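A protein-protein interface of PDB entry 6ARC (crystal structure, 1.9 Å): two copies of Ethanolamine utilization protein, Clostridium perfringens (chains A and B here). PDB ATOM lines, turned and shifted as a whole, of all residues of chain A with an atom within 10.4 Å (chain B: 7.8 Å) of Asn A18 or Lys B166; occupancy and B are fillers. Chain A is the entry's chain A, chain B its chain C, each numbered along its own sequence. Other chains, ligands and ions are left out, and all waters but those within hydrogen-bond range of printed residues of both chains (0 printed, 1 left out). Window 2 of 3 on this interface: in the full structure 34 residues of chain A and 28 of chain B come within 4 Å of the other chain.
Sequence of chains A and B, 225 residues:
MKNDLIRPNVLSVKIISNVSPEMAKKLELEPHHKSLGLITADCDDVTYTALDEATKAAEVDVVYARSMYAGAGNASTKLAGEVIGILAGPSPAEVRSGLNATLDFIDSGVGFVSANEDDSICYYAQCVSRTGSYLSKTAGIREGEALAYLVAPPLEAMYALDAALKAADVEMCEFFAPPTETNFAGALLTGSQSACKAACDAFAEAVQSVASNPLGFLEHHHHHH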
ATOM      1  N   ILE A  15     -10.807 -20.354  -9.770  1.00  0.00           N
ATOM      2  CA  ILE A  15      -9.955 -21.014 -10.761  1.00  0.00           C
ATOM      3  C   ILE A  15     -10.136 -20.341 -12.114  1.00  0.00           C
ATOM      4  O   ILE A  15     -11.262 -20.067 -12.537  1.00  0.00           O
ATOM      5  CB  ILE A  15     -10.264 -22.511 -10.885  1.00  0.00           C
ATOM      6  CG1 ILE A  15      -9.907 -23.226  -9.586  1.00  0.00           C
ATOM      7  CG2 ILE A  15      -9.451 -23.104 -12.026  1.00  0.00           C
ATOM      8  CD1 ILE A  15     -10.328 -24.690  -9.557  1.00  0.00           C
ATOM      9  N   ILE A  16      -9.024 -20.112 -12.800  1.00  0.00           N
ATOM     10  CA  ILE A  16      -9.013 -19.661 -14.182  1.00  0.00           C
ATOM     11  C   ILE A  16      -8.537 -20.830 -15.025  1.00  0.00           C
ATOM     12  O   ILE A  16      -7.408 -21.312 -14.847  1.00  0.00           O
ATOM     13  CB  ILE A  16      -8.093 -18.445 -14.392  1.00  0.00           C
ATOM     14  CG1 ILE A  16      -8.625 -17.200 -13.660  1.00  0.00           C
ATOM     15  CG2 ILE A  16      -7.939 -18.113 -15.902  1.00  0.00           C
ATOM     16  CD1 ILE A  16      -7.615 -16.083 -13.576  1.00  0.00           C
ATOM     17  N   SER A  17      -9.402 -21.310 -15.917  1.00  0.00           N
ATOM     18  CA  SER A  17      -9.007 -22.274 -16.928  1.00  0.00           C
ATOM     19  C   SER A  17      -8.542 -21.509 -18.160  1.00  0.00           C
ATOM     20  O   SER A  17      -9.175 -20.530 -18.578  1.00  0.00           O
ATOM     21  CB  SER A  17     -10.174 -23.200 -17.292  1.00  0.00           C
ATOM     22  OG  SER A  17     -10.776 -23.770 -16.138  1.00  0.00           O
ATOM     23  N   ASN A  18      -7.420 -21.939 -18.725  1.00  0.00           N
ATOM     24  CA  ASN A  18      -6.941 -21.412 -19.998  1.00  0.00           C
ATOM     25  C   ASN A  18      -6.589 -19.930 -19.858  1.00  0.00           C
ATOM     26  O   ASN A  18      -7.159 -19.063 -20.524  1.00  0.00           O
ATOM     27  CB  ASN A  18      -7.989 -21.643 -21.102  1.00  0.00           C
ATOM     28  CG  ASN A  18      -7.561 -21.092 -22.479  1.00  0.00           C
ATOM     29  OD1 ASN A  18      -6.418 -21.268 -22.906  1.00  0.00           O
ATOM     30  ND2 ASN A  18      -8.491 -20.434 -23.174  1.00  0.00           N
ATOM     31  N   VAL A  19      -5.615 -19.644 -18.988  1.00  0.00           N
ATOM     32  CA  VAL A  19      -5.309 -18.245 -18.730  1.00  0.00           C
ATOM     33  C   VAL A  19      -4.940 -17.574 -20.037  1.00  0.00           C
ATOM     34  O   VAL A  19      -4.295 -18.172 -20.899  1.00  0.00           O
ATOM     35  CB  VAL A  19      -4.185 -18.155 -17.684  1.00  0.00           C
ATOM     36  CG1 VAL A  19      -2.920 -18.831 -18.204  1.00  0.00           C
ATOM     37  CG2 VAL A  19      -3.944 -16.740 -17.283  1.00  0.00           C
ATOM     38  N   SER A  20      -5.367 -16.321 -20.195  1.00  0.00           N
ATOM     39  CA  SER A  20      -5.082 -15.575 -21.406  1.00  0.00           C
ATOM     40  C   SER A  20      -3.572 -15.367 -21.574  1.00  0.00           C
ATOM     41  O   SER A  20      -2.837 -15.225 -20.592  1.00  0.00           O
ATOM     42  CB  SER A  20      -5.812 -14.232 -21.371  1.00  0.00           C
ATOM     43  OG  SER A  20      -5.340 -13.479 -20.278  1.00  0.00           O
ATOM     44  N   PRO A  21      -3.075 -15.341 -22.811  1.00  0.00           N
ATOM     45  CA  PRO A  21      -1.624 -15.146 -22.996  1.00  0.00           C
ATOM     46  C   PRO A  21      -1.093 -13.852 -22.399  1.00  0.00           C
ATOM     47  O   PRO A  21       0.032 -13.838 -21.892  1.00  0.00           O
ATOM     48  CB  PRO A  21      -1.454 -15.167 -24.518  1.00  0.00           C
ATOM     49  CG  PRO A  21      -2.693 -15.848 -25.037  1.00  0.00           C
ATOM     50  CD  PRO A  21      -3.786 -15.527 -24.093  1.00  0.00           C
ATOM     51  N   GLU A  22      -1.856 -12.760 -22.470  1.00  0.00           N
ATOM     52  CA  GLU A  22      -1.386 -11.490 -21.923  1.00  0.00           C
ATOM     53  C   GLU A  22      -1.142 -11.600 -20.422  1.00  0.00           C
ATOM     54  O   GLU A  22      -0.140 -11.085 -19.906  1.00  0.00           O
ATOM     55  CB  GLU A  22      -2.397 -10.371 -22.210  1.00  0.00           C
ATOM     56  CG  GLU A  22      -2.607 -10.041 -23.703  1.00  0.00           C
ATOM     57  CD  GLU A  22      -3.523 -11.040 -24.413  1.00  0.00           C
ATOM     58  OE1 GLU A  22      -3.745 -10.861 -25.632  1.00  0.00           O
ATOM     59  OE2 GLU A  22      -4.023 -12.000 -23.763  1.00  0.00           O
ATOM     60  N   MET A  23      -2.047 -12.272 -19.707  1.00  0.00           N
ATOM     61  CA  MET A  23      -1.872 -12.447 -18.267  1.00  0.00           C
ATOM     62  C   MET A  23      -0.735 -13.412 -17.967  1.00  0.00           C
ATOM     63  O   MET A  23       0.071 -13.166 -17.062  1.00  0.00           O
ATOM     64  CB  MET A  23      -3.175 -12.941 -17.638  1.00  0.00           C
ATOM     65  CG  MET A  23      -4.318 -11.936 -17.712  1.00  0.00           C
ATOM     66  SD  MET A  23      -3.974 -10.420 -16.790  1.00  0.00           S
ATOM     67  CE  MET A  23      -3.830 -11.029 -15.118  1.00  0.00           C
ATOM     68  N   ALA A  24      -0.657 -14.524 -18.710  1.00  0.00           N
ATOM     69  CA  ALA A  24       0.495 -15.417 -18.587  1.00  0.00           C
ATOM     70  C   ALA A  24       1.804 -14.649 -18.715  1.00  0.00           C
ATOM     71  O   ALA A  24       2.780 -14.939 -18.013  1.00  0.00           O
ATOM     72  CB  ALA A  24       0.447 -16.514 -19.662  1.00  0.00           C
ATOM     73  N   LEU A  27       2.350 -12.318 -15.615  1.00  0.00           N
ATOM     74  CA  LEU A  27       2.648 -13.154 -14.465  1.00  0.00           C
ATOM     75  C   LEU A  27       3.886 -14.014 -14.666  1.00  0.00           C
ATOM     76  O   LEU A  27       4.254 -14.769 -13.760  1.00  0.00           O
ATOM     77  CB  LEU A  27       1.456 -14.062 -14.165  1.00  0.00           C
ATOM     78  CG  LEU A  27       0.183 -13.355 -13.716  1.00  0.00           C
ATOM     79  CD1 LEU A  27      -0.947 -14.371 -13.568  1.00  0.00           C
ATOM     80  CD2 LEU A  27       0.446 -12.626 -12.409  1.00  0.00           C
ATOM     81  N   LEU A  29       4.489 -16.690 -16.360  1.00  0.00           N
ATOM     82  CA  LEU A  29       4.229 -18.108 -16.208  1.00  0.00           C
ATOM     83  C   LEU A  29       5.127 -18.916 -17.127  1.00  0.00           C
ATOM     84  O   LEU A  29       5.595 -18.441 -18.164  1.00  0.00           O
ATOM     85  CB  LEU A  29       2.775 -18.437 -16.542  1.00  0.00           C
ATOM     86  CG  LEU A  29       1.709 -17.663 -15.780  1.00  0.00           C
ATOM     87  CD1 LEU A  29       0.375 -18.216 -16.163  1.00  0.00           C
ATOM     88  CD2 LEU A  29       1.931 -17.783 -14.274  1.00  0.00           C
ATOM     89  N   PRO A  31       5.582 -22.191 -19.740  1.00  0.00           N
ATOM     90  CA  PRO A  31       4.716 -22.652 -20.846  1.00  0.00           C
ATOM     91  C   PRO A  31       3.677 -23.692 -20.454  1.00  0.00           C
ATOM     92  O   PRO A  31       2.590 -23.712 -21.042  1.00  0.00           O
ATOM     93  CB  PRO A  31       5.724 -23.238 -21.840  1.00  0.00           C
ATOM     94  CG  PRO A  31       6.998 -22.498 -21.564  1.00  0.00           C
ATOM     95  CD  PRO A  31       7.014 -22.269 -20.087  1.00  0.00           C
ATOM     96  N   HIS A  32       3.971 -24.564 -19.493  1.00  0.00           N
ATOM     97  CA  HIS A  32       3.031 -25.619 -19.129  1.00  0.00           C
ATOM     98  C   HIS A  32       1.978 -25.175 -18.115  1.00  0.00           C
ATOM     99  O   HIS A  32       1.096 -25.973 -17.791  1.00  0.00           O
ATOM    100  CB  HIS A  32       3.789 -26.836 -18.579  1.00  0.00           C
ATOM    101  CG  HIS A  32       4.424 -26.603 -17.242  1.00  0.00           C
ATOM    102  ND1 HIS A  32       5.527 -25.791 -17.074  1.00  0.00           N
ATOM    103  CD2 HIS A  32       4.094 -27.049 -16.006  1.00  0.00           C
ATOM    104  CE1 HIS A  32       5.862 -25.766 -15.796  1.00  0.00           C
ATOM    105  NE2 HIS A  32       5.007 -26.518 -15.126  1.00  0.00           N
ATOM    106  N   HIS A  33       2.010 -23.918 -17.666  1.00  0.00           N
ATOM    107  CA  HIS A  33       1.018 -23.348 -16.741  1.00  0.00           C
ATOM    108  C   HIS A  33      -0.230 -22.947 -17.531  1.00  0.00           C
ATOM    109  O   HIS A  33      -0.273 -21.886 -18.157  1.00  0.00           O
ATOM    110  CB  HIS A  33       1.605 -22.120 -16.053  1.00  0.00           C
ATOM    111  CG  HIS A  33       2.680 -22.408 -15.037  1.00  0.00           C
ATOM    112  ND1 HIS A  33       3.570 -21.440 -14.610  1.00  0.00           N
ATOM    113  CD2 HIS A  33       2.953 -23.513 -14.299  1.00  0.00           C
ATOM    114  CE1 HIS A  33       4.374 -21.951 -13.693  1.00  0.00           C
ATOM    115  NE2 HIS A  33       4.015 -23.203 -13.478  1.00  0.00           N
ATOM    116  N   LYS A  34      -1.245 -23.796 -17.537  1.00  0.00           N
ATOM    117  CA  LYS A  34      -2.477 -23.513 -18.271  1.00  0.00           C
ATOM    118  C   LYS A  34      -3.561 -22.887 -17.405  1.00  0.00           C
ATOM    119  O   LYS A  34      -4.391 -22.132 -17.917  1.00  0.00           O
ATOM    120  CB  LYS A  34      -3.037 -24.804 -18.886  1.00  0.00           C
ATOM    121  CG  LYS A  34      -2.056 -25.558 -19.788  1.00  0.00           C
ATOM    122  CD  LYS A  34      -1.737 -24.711 -21.023  1.00  0.00           C
ATOM    123  CE  LYS A  34      -0.923 -25.467 -22.063  1.00  0.00           C
ATOM    124  NZ  LYS A  34      -0.605 -24.596 -23.225  1.00  0.00           N
ATOM    125  N   SER A  35      -3.592 -23.218 -16.121  1.00  0.00           N
ATOM    126  CA  SER A  35      -4.678 -22.847 -15.226  1.00  0.00           C
ATOM    127  C   SER A  35      -4.102 -22.156 -14.003  1.00  0.00           C
ATOM    128  O   SER A  35      -2.992 -22.462 -13.574  1.00  0.00           O
ATOM    129  CB  SER A  35      -5.484 -24.076 -14.777  1.00  0.00           C
ATOM    130  OG  SER A  35      -5.774 -24.914 -15.907  1.00  0.00           O
ATOM    131  N   LEU A  36      -4.894 -21.268 -13.423  1.00  0.00           N
ATOM    132  CA  LEU A  36      -4.507 -20.542 -12.224  1.00  0.00           C
ATOM    133  C   LEU A  36      -5.515 -20.819 -11.121  1.00  0.00           C
ATOM    134  O   LEU A  36      -6.712 -20.971 -11.372  1.00  0.00           O
ATOM    135  CB  LEU A  36      -4.439 -19.016 -12.483  1.00  0.00           C
ATOM    136  CG  LEU A  36      -3.407 -18.604 -13.532  1.00  0.00           C
ATOM    137  CD1 LEU A  36      -3.436 -17.087 -13.723  1.00  0.00           C
ATOM    138  CD2 LEU A  36      -2.019 -19.031 -13.165  1.00  0.00           C
ATOM    139  N   GLY A  37      -5.013 -20.875  -9.898  1.00  0.00           N
ATOM    140  CA  GLY A  37      -5.864 -20.882  -8.738  1.00  0.00           C
ATOM    141  C   GLY A  37      -5.553 -19.649  -7.905  1.00  0.00           C
ATOM    142  O   GLY A  37      -4.409 -19.466  -7.478  1.00  0.00           O
ATOM    143  N   LEU A  87      -1.630 -19.989  -7.509  1.00  0.00           N
ATOM    144  CA  LEU A  87      -1.035 -21.255  -7.916  1.00  0.00           C
ATOM    145  C   LEU A  87      -1.201 -21.410  -9.428  1.00  0.00           C
ATOM    146  O   LEU A  87      -2.229 -21.019  -9.988  1.00  0.00           O
ATOM    147  CB  LEU A  87      -1.721 -22.413  -7.183  1.00  0.00           C
ATOM    148  CG  LEU A  87      -1.598 -22.571  -5.662  1.00  0.00           C
ATOM    149  CD1 LEU A  87      -2.524 -23.702  -5.180  1.00  0.00           C
ATOM    150  CD2 LEU A  87      -0.131 -22.867  -5.255  1.00  0.00           C
ATOM    151  N   ALA A  88      -0.197 -21.967 -10.097  1.00  0.00           N
ATOM    152  CA  ALA A  88      -0.334 -22.288 -11.514  1.00  0.00           C
ATOM    153  C   ALA A  88      -0.105 -23.787 -11.693  1.00  0.00           C
ATOM    154  O   ALA A  88       0.760 -24.373 -11.046  1.00  0.00           O
ATOM    155  CB  ALA A  88       0.649 -21.505 -12.373  1.00  0.00           C
ATOM    156  N   GLY A  89      -0.872 -24.395 -12.575  1.00  0.00           N
ATOM    157  CA  GLY A  89      -0.762 -25.816 -12.790  1.00  0.00           C
ATOM    158  C   GLY A  89      -1.129 -26.162 -14.205  1.00  0.00           C
ATOM    159  O   GLY A  89      -1.492 -25.300 -15.002  1.00  0.00           O
ATOM    160  N   PRO A  90      -0.991 -27.445 -14.540  1.00  0.00           N
ATOM    161  CA  PRO A  90      -1.262 -27.897 -15.920  1.00  0.00           C
ATOM    162  C   PRO A  90      -2.718 -27.926 -16.299  1.00  0.00           C
ATOM    163  O   PRO A  90      -3.008 -28.004 -17.504  1.00  0.00           O
ATOM    164  CB  PRO A  90      -0.696 -29.330 -15.952  1.00  0.00           C
ATOM    165  CG  PRO A  90      -0.711 -29.800 -14.529  1.00  0.00           C
ATOM    166  CD  PRO A  90      -0.513 -28.535 -13.663  1.00  0.00           C
ATOM    167  N   SER A  91      -3.637 -27.998 -15.339  1.00  0.00           N
ATOM    168  CA  SER A  91      -5.052 -28.163 -15.653  1.00  0.00           C
ATOM    169  C   SER A  91      -5.892 -27.596 -14.527  1.00  0.00           C
ATOM    170  O   SER A  91      -5.414 -27.486 -13.390  1.00  0.00           O
ATOM    171  CB  SER A  91      -5.402 -29.647 -15.820  1.00  0.00           C
ATOM    172  OG  SER A  91      -5.463 -30.271 -14.539  1.00  0.00           O
ATOM    173  N   PRO A  92      -7.182 -27.348 -14.777  1.00  0.00           N
ATOM    174  CA  PRO A  92      -8.060 -26.910 -13.686  1.00  0.00           C
ATOM    175  C   PRO A  92      -8.177 -27.953 -12.587  1.00  0.00           C
ATOM    176  O   PRO A  92      -8.385 -27.607 -11.414  1.00  0.00           O
ATOM    177  CB  PRO A  92      -9.409 -26.694 -14.384  1.00  0.00           C
ATOM    178  CG  PRO A  92      -9.107 -26.573 -15.826  1.00  0.00           C
ATOM    179  CD  PRO A  92      -7.903 -27.426 -16.061  1.00  0.00           C
ATOM    180  N   ALA A  93      -8.054 -29.234 -12.932  1.00  0.00           N
ATOM    181  CA  ALA A  93      -8.188 -30.285 -11.921  1.00  0.00           C
ATOM    182  C   ALA A  93      -6.993 -30.304 -10.977  1.00  0.00           C
ATOM    183  O   ALA A  93      -7.151 -30.451  -9.760  1.00  0.00           O
ATOM    184  CB  ALA A  93      -8.367 -31.658 -12.584  1.00  0.00           C
ATOM    185  N   VAL A  95      -4.967 -27.787 -10.403  1.00  0.00           N
ATOM    186  CA  VAL A  95      -5.073 -26.562  -9.610  1.00  0.00           C
ATOM    187  C   VAL A  95      -6.073 -26.739  -8.475  1.00  0.00           C
ATOM    188  O   VAL A  95      -5.811 -26.337  -7.333  1.00  0.00           O
ATOM    189  CB  VAL A  95      -5.446 -25.370 -10.512  1.00  0.00           C
ATOM    190  CG1 VAL A  95      -5.948 -24.179  -9.697  1.00  0.00           C
ATOM    191  CG2 VAL A  95      -4.262 -24.982 -11.350  1.00  0.00           C
ATOM    192  N   TYR B 159      -9.103 -12.162 -11.863  1.00  0.00           N
ATOM    193  CA  TYR B 159     -10.124 -12.987 -12.492  1.00  0.00           C
ATOM    194  C   TYR B 159     -10.818 -12.231 -13.620  1.00  0.00           C
ATOM    195  O   TYR B 159     -11.092 -12.786 -14.693  1.00  0.00           O
ATOM    196  CB  TYR B 159     -11.129 -13.390 -11.421  1.00  0.00           C
ATOM    197  CG  TYR B 159     -12.215 -14.332 -11.873  1.00  0.00           C
ATOM    198  CD1 TYR B 159     -11.979 -15.707 -11.901  1.00  0.00           C
ATOM    199  CD2 TYR B 159     -13.470 -13.870 -12.252  1.00  0.00           C
ATOM    200  CE1 TYR B 159     -12.954 -16.594 -12.289  1.00  0.00           C
ATOM    201  CE2 TYR B 159     -14.454 -14.751 -12.663  1.00  0.00           C
ATOM    202  CZ  TYR B 159     -14.185 -16.126 -12.671  1.00  0.00           C
ATOM    203  OH  TYR B 159     -15.123 -17.062 -13.058  1.00  0.00           O
ATOM    204  N   ALA B 160     -11.192 -10.986 -13.358  1.00  0.00           N
ATOM    205  CA  ALA B 160     -11.971 -10.218 -14.321  1.00  0.00           C
ATOM    206  C   ALA B 160     -11.120  -9.680 -15.461  1.00  0.00           C
ATOM    207  O   ALA B 160     -11.643  -9.490 -16.564  1.00  0.00           O
ATOM    208  CB  ALA B 160     -12.705  -9.092 -13.593  1.00  0.00           C
ATOM    209  N   LEU B 161      -9.823  -9.431 -15.227  1.00  0.00           N
ATOM    210  CA  LEU B 161      -8.931  -9.063 -16.322  1.00  0.00           C
ATOM    211  C   LEU B 161      -8.842 -10.194 -17.335  1.00  0.00           C
ATOM    212  O   LEU B 161      -8.885  -9.965 -18.551  1.00  0.00           O
ATOM    213  CB  LEU B 161      -7.537  -8.704 -15.797  1.00  0.00           C
ATOM    214  CG  LEU B 161      -7.353  -7.314 -15.187  1.00  0.00           C
ATOM    215  CD1 LEU B 161      -5.889  -7.153 -14.766  1.00  0.00           C
ATOM    216  CD2 LEU B 161      -7.771  -6.168 -16.145  1.00  0.00           C
ATOM    217  N   ASP B 162      -8.733 -11.431 -16.849  1.00  0.00           N
ATOM    218  CA  ASP B 162      -8.738 -12.569 -17.755  1.00  0.00           C
ATOM    219  C   ASP B 162     -10.041 -12.619 -18.557  1.00  0.00           C
ATOM    220  O   ASP B 162     -10.016 -12.802 -19.778  1.00  0.00           O
ATOM    221  CB  ASP B 162      -8.513 -13.857 -16.960  1.00  0.00           C
ATOM    222  CG  ASP B 162      -8.374 -15.077 -17.864  1.00  0.00           C
ATOM    223  OD1 ASP B 162      -7.302 -15.199 -18.511  1.00  0.00           O
ATOM    224  OD2 ASP B 162      -9.338 -15.865 -17.943  1.00  0.00           O
ATOM    225  N   ALA B 163     -11.182 -12.388 -17.908  1.00  0.00           N
ATOM    226  CA  ALA B 163     -12.449 -12.364 -18.634  1.00  0.00           C
ATOM    227  C   ALA B 163     -12.472 -11.256 -19.686  1.00  0.00           C
ATOM    228  O   ALA B 163     -12.915 -11.477 -20.821  1.00  0.00           O
ATOM    229  CB  ALA B 163     -13.620 -12.202 -17.655  1.00  0.00           C
ATOM    230  N   ALA B 164     -11.972 -10.065 -19.335  1.00  0.00           N
ATOM    231  CA  ALA B 164     -11.973  -8.939 -20.264  1.00  0.00           C
ATOM    232  C   ALA B 164     -11.105  -9.211 -21.485  1.00  0.00           C
ATOM    233  O   ALA B 164     -11.479  -8.867 -22.613  1.00  0.00           O
ATOM    234  CB  ALA B 164     -11.474  -7.689 -19.528  1.00  0.00           C
ATOM    235  N   LEU B 165      -9.934  -9.801 -21.283  1.00  0.00           N
ATOM    236  CA  LEU B 165      -9.040 -10.054 -22.399  1.00  0.00           C
ATOM    237  C   LEU B 165      -9.617 -11.109 -23.330  1.00  0.00           C
ATOM    238  O   LEU B 165      -9.459 -11.019 -24.548  1.00  0.00           O
ATOM    239  CB  LEU B 165      -7.670 -10.491 -21.882  1.00  0.00           C
ATOM    240  CG  LEU B 165      -6.826  -9.383 -21.214  1.00  0.00           C
ATOM    241  CD1 LEU B 165      -5.760  -9.979 -20.254  1.00  0.00           C
ATOM    242  CD2 LEU B 165      -6.187  -8.486 -22.237  1.00  0.00           C
ATOM    243  N   LYS B 166     -10.340 -12.078 -22.780  1.00  0.00           N
ATOM    244  CA  LYS B 166     -10.957 -13.095 -23.618  1.00  0.00           C
ATOM    245  C   LYS B 166     -12.174 -12.579 -24.364  1.00  0.00           C
ATOM    246  O   LYS B 166     -12.502 -13.103 -25.430  1.00  0.00           O
ATOM    247  CB  LYS B 166     -11.337 -14.297 -22.763  1.00  0.00           C
ATOM    248  CG  LYS B 166     -10.142 -15.053 -22.266  1.00  0.00           C
ATOM    249  CD  LYS B 166     -10.543 -16.101 -21.251  1.00  0.00           C
ATOM    250  CE  LYS B 166      -9.339 -16.938 -20.853  1.00  0.00           C
ATOM    251  NZ  LYS B 166      -9.699 -17.801 -19.745  1.00  0.00           N
ATOM    252  N   ALA B 167     -12.842 -11.556 -23.849  1.00  0.00           N
ATOM    253  CA  ALA B 167     -14.116 -11.134 -24.413  1.00  0.00           C
ATOM    254  C   ALA B 167     -13.985 -10.154 -25.573  1.00  0.00           C
ATOM    255  O   ALA B 167     -14.973  -9.926 -26.287  1.00  0.00           O
ATOM    256  CB  ALA B 167     -14.985 -10.499 -23.330  1.00  0.00           C
ATOM    257  N   ALA B 168     -12.822  -9.549 -25.767  1.00  0.00           N
ATOM    258  CA  ALA B 168     -12.724  -8.458 -26.730  1.00  0.00           C
ATOM    259  C   ALA B 168     -11.343  -8.422 -27.368  1.00  0.00           C
ATOM    260  O   ALA B 168     -10.370  -8.994 -26.866  1.00  0.00           O
ATOM    261  CB  ALA B 168     -13.051  -7.119 -26.080  1.00  0.00           C
ATOM    262  N   ASP B 169     -11.278  -7.732 -28.497  1.00  0.00           N
ATOM    263  CA  ASP B 169     -10.046  -7.594 -29.260  1.00  0.00           C
ATOM    264  C   ASP B 169      -9.241  -6.418 -28.693  1.00  0.00           C
ATOM    265  O   ASP B 169      -9.182  -5.321 -29.249  1.00  0.00           O
ATOM    266  CB  ASP B 169     -10.395  -7.432 -30.735  1.00  0.00           C
ATOM    267  CG  ASP B 169      -9.211  -7.582 -31.634  1.00  0.00           C
ATOM    268  OD1 ASP B 169      -8.094  -7.773 -31.106  1.00  0.00           O
ATOM    269  OD2 ASP B 169      -9.415  -7.549 -32.878  1.00  0.00           O
ATOM    270  N   VAL B 170      -8.651  -6.665 -27.519  1.00  0.00           N
ATOM    271  CA  VAL B 170      -7.907  -5.655 -26.769  1.00  0.00           C
ATOM    272  C   VAL B 170      -6.537  -6.209 -26.378  1.00  0.00           C
ATOM    273  O   VAL B 170      -6.335  -7.424 -26.278  1.00  0.00           O
ATOM    274  CB  VAL B 170      -8.669  -5.199 -25.494  1.00  0.00           C
ATOM    275  CG1 VAL B 170      -9.933  -4.388 -25.845  1.00  0.00           C
ATOM    276  CG2 VAL B 170      -9.025  -6.389 -24.605  1.00  0.00           C
ATOM    277  N   LEU B 189      -6.265  -1.392 -20.881  1.00  0.00           N
ATOM    278  CA  LEU B 189      -6.341  -2.168 -22.114  1.00  0.00           C
ATOM    279  C   LEU B 189      -6.731  -1.243 -23.258  1.00  0.00           C
ATOM    280  O   LEU B 189      -7.473  -0.276 -23.059  1.00  0.00           O
ATOM    281  CB  LEU B 189      -7.369  -3.308 -22.022  1.00  0.00           C
ATOM    282  CG  LEU B 189      -7.390  -4.198 -20.774  1.00  0.00           C
ATOM    283  CD1 LEU B 189      -8.447  -5.281 -20.907  1.00  0.00           C
ATOM    284  CD2 LEU B 189      -6.034  -4.822 -20.508  1.00  0.00           C
ATOM    285  N   ALA B 199     -14.686  -4.998 -23.355  1.00  0.00           N
ATOM    286  CA  ALA B 199     -13.820  -5.381 -22.246  1.00  0.00           C
ATOM    287  C   ALA B 199     -14.350  -4.852 -20.912  1.00  0.00           C
ATOM    288  O   ALA B 199     -14.341  -5.572 -19.907  1.00  0.00           O
ATOM    289  CB  ALA B 199     -12.391  -4.882 -22.490  1.00  0.00           C
ATOM    290  N   ALA B 202     -17.363  -6.989 -19.818  1.00  0.00           N
ATOM    291  CA  ALA B 202     -16.928  -8.302 -19.353  1.00  0.00           C
ATOM    292  C   ALA B 202     -16.231  -8.206 -18.002  1.00  0.00           C
ATOM    293  O   ALA B 202     -16.412  -9.074 -17.134  1.00  0.00           O
ATOM    294  CB  ALA B 202     -16.007  -8.941 -20.391  1.00  0.00           C
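NZ of Lys B166 lies within hydrogen-bond range of O of Ser A17 (3.0 Å).
The backbone carbonyl oxygen (O) of Asn A18 is in hydrogen-bond range of the side-chain amino group (NZ) of Lys B166, at 2.9 Å.
N of Ser A20 is in hydrogen-bond range of OD1 of Asp B162 (2.8 Å).
O of Leu A36 sits at hydrogen-bond distance from N of Ile A16 (2.8 Å).
N of Asn A18 sits at hydrogen-bond distance from O of Lys A34.
O of Lys A34 lies within hydrogen-bond range of N of Val A19 (3.0 Å).
The side-chain amino group (NZ) of Lys B166 lies within salt-bridge range of the side-chain carboxylate (OD2) of Asp B162.
No position is printed for both chains.
Of the 9 pairs that touch across the chains among the printed residues, none has its exchanged pair printed and touching as well.
Among the printed residues, pairs that only touch across the chains: Ile A15 with Tyr B159, Ile A16 with Asp B162, Val A19 with Asp B162, Ser A20 with Leu B165, Glu A22 with Leu B165 and Met A23 with Leu B165.
Of the 27 printed residues of chain A, 8 touch a printed residue of chain B.
Hydrophobic or aromatic side chains of chain A within 4 Å of the printed part of chain B: Ile A16, Val A19 and Met A23.
Along chain A the printed residues that touch a printed residue of chain B span positions 15 to 23.
Of the 15 printed residues of chain B, 4 touch a printed residue of chain A.
Hydrophobic or aromatic side chains of chain B within 4 Å of the printed part of chain A: Tyr B159 and Leu B165.
Among the printed residues, no Asp or Glu carboxylate lies within 4 Å of a Lys or Arg side-chain nitrogen of the other chain.
Printed residues of chain B within 4 Å of Asn A18: Lys B166.
Printed residues of chain A within 4 Å of Lys B166: Ser A17 (3.0 Å) and Asn A18 (2.9 Å).
No residue of chain A comes within 4 Å of Ala B163.
No residue of chain A comes within 4 Å of Ala B164.
No residue of chain A comes within 4 Å of Ala B167.
No residue of chain A comes within 4 Å of Ala B168.
Of the printed residues of chain B, Ser A20 touches Asp B162 (2.8 Å) and Leu B165 (3.5 Å).
Of the printed residues of chain B, Val A19 touches Asp B162.
Of the printed residues of chain B, Ile A16 touches Asp B162 (3.3 Å).
Printed residues of chain B within 4 Å of Glu A22: Leu B165 (3.9 Å).
The nearest printed residue of chain A that does not touch Lys B166 is Ser A20 (4.1 Å).
The nearest printed residue of chain B that does not touch Val A19 is Lys B166 (4.5 Å).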
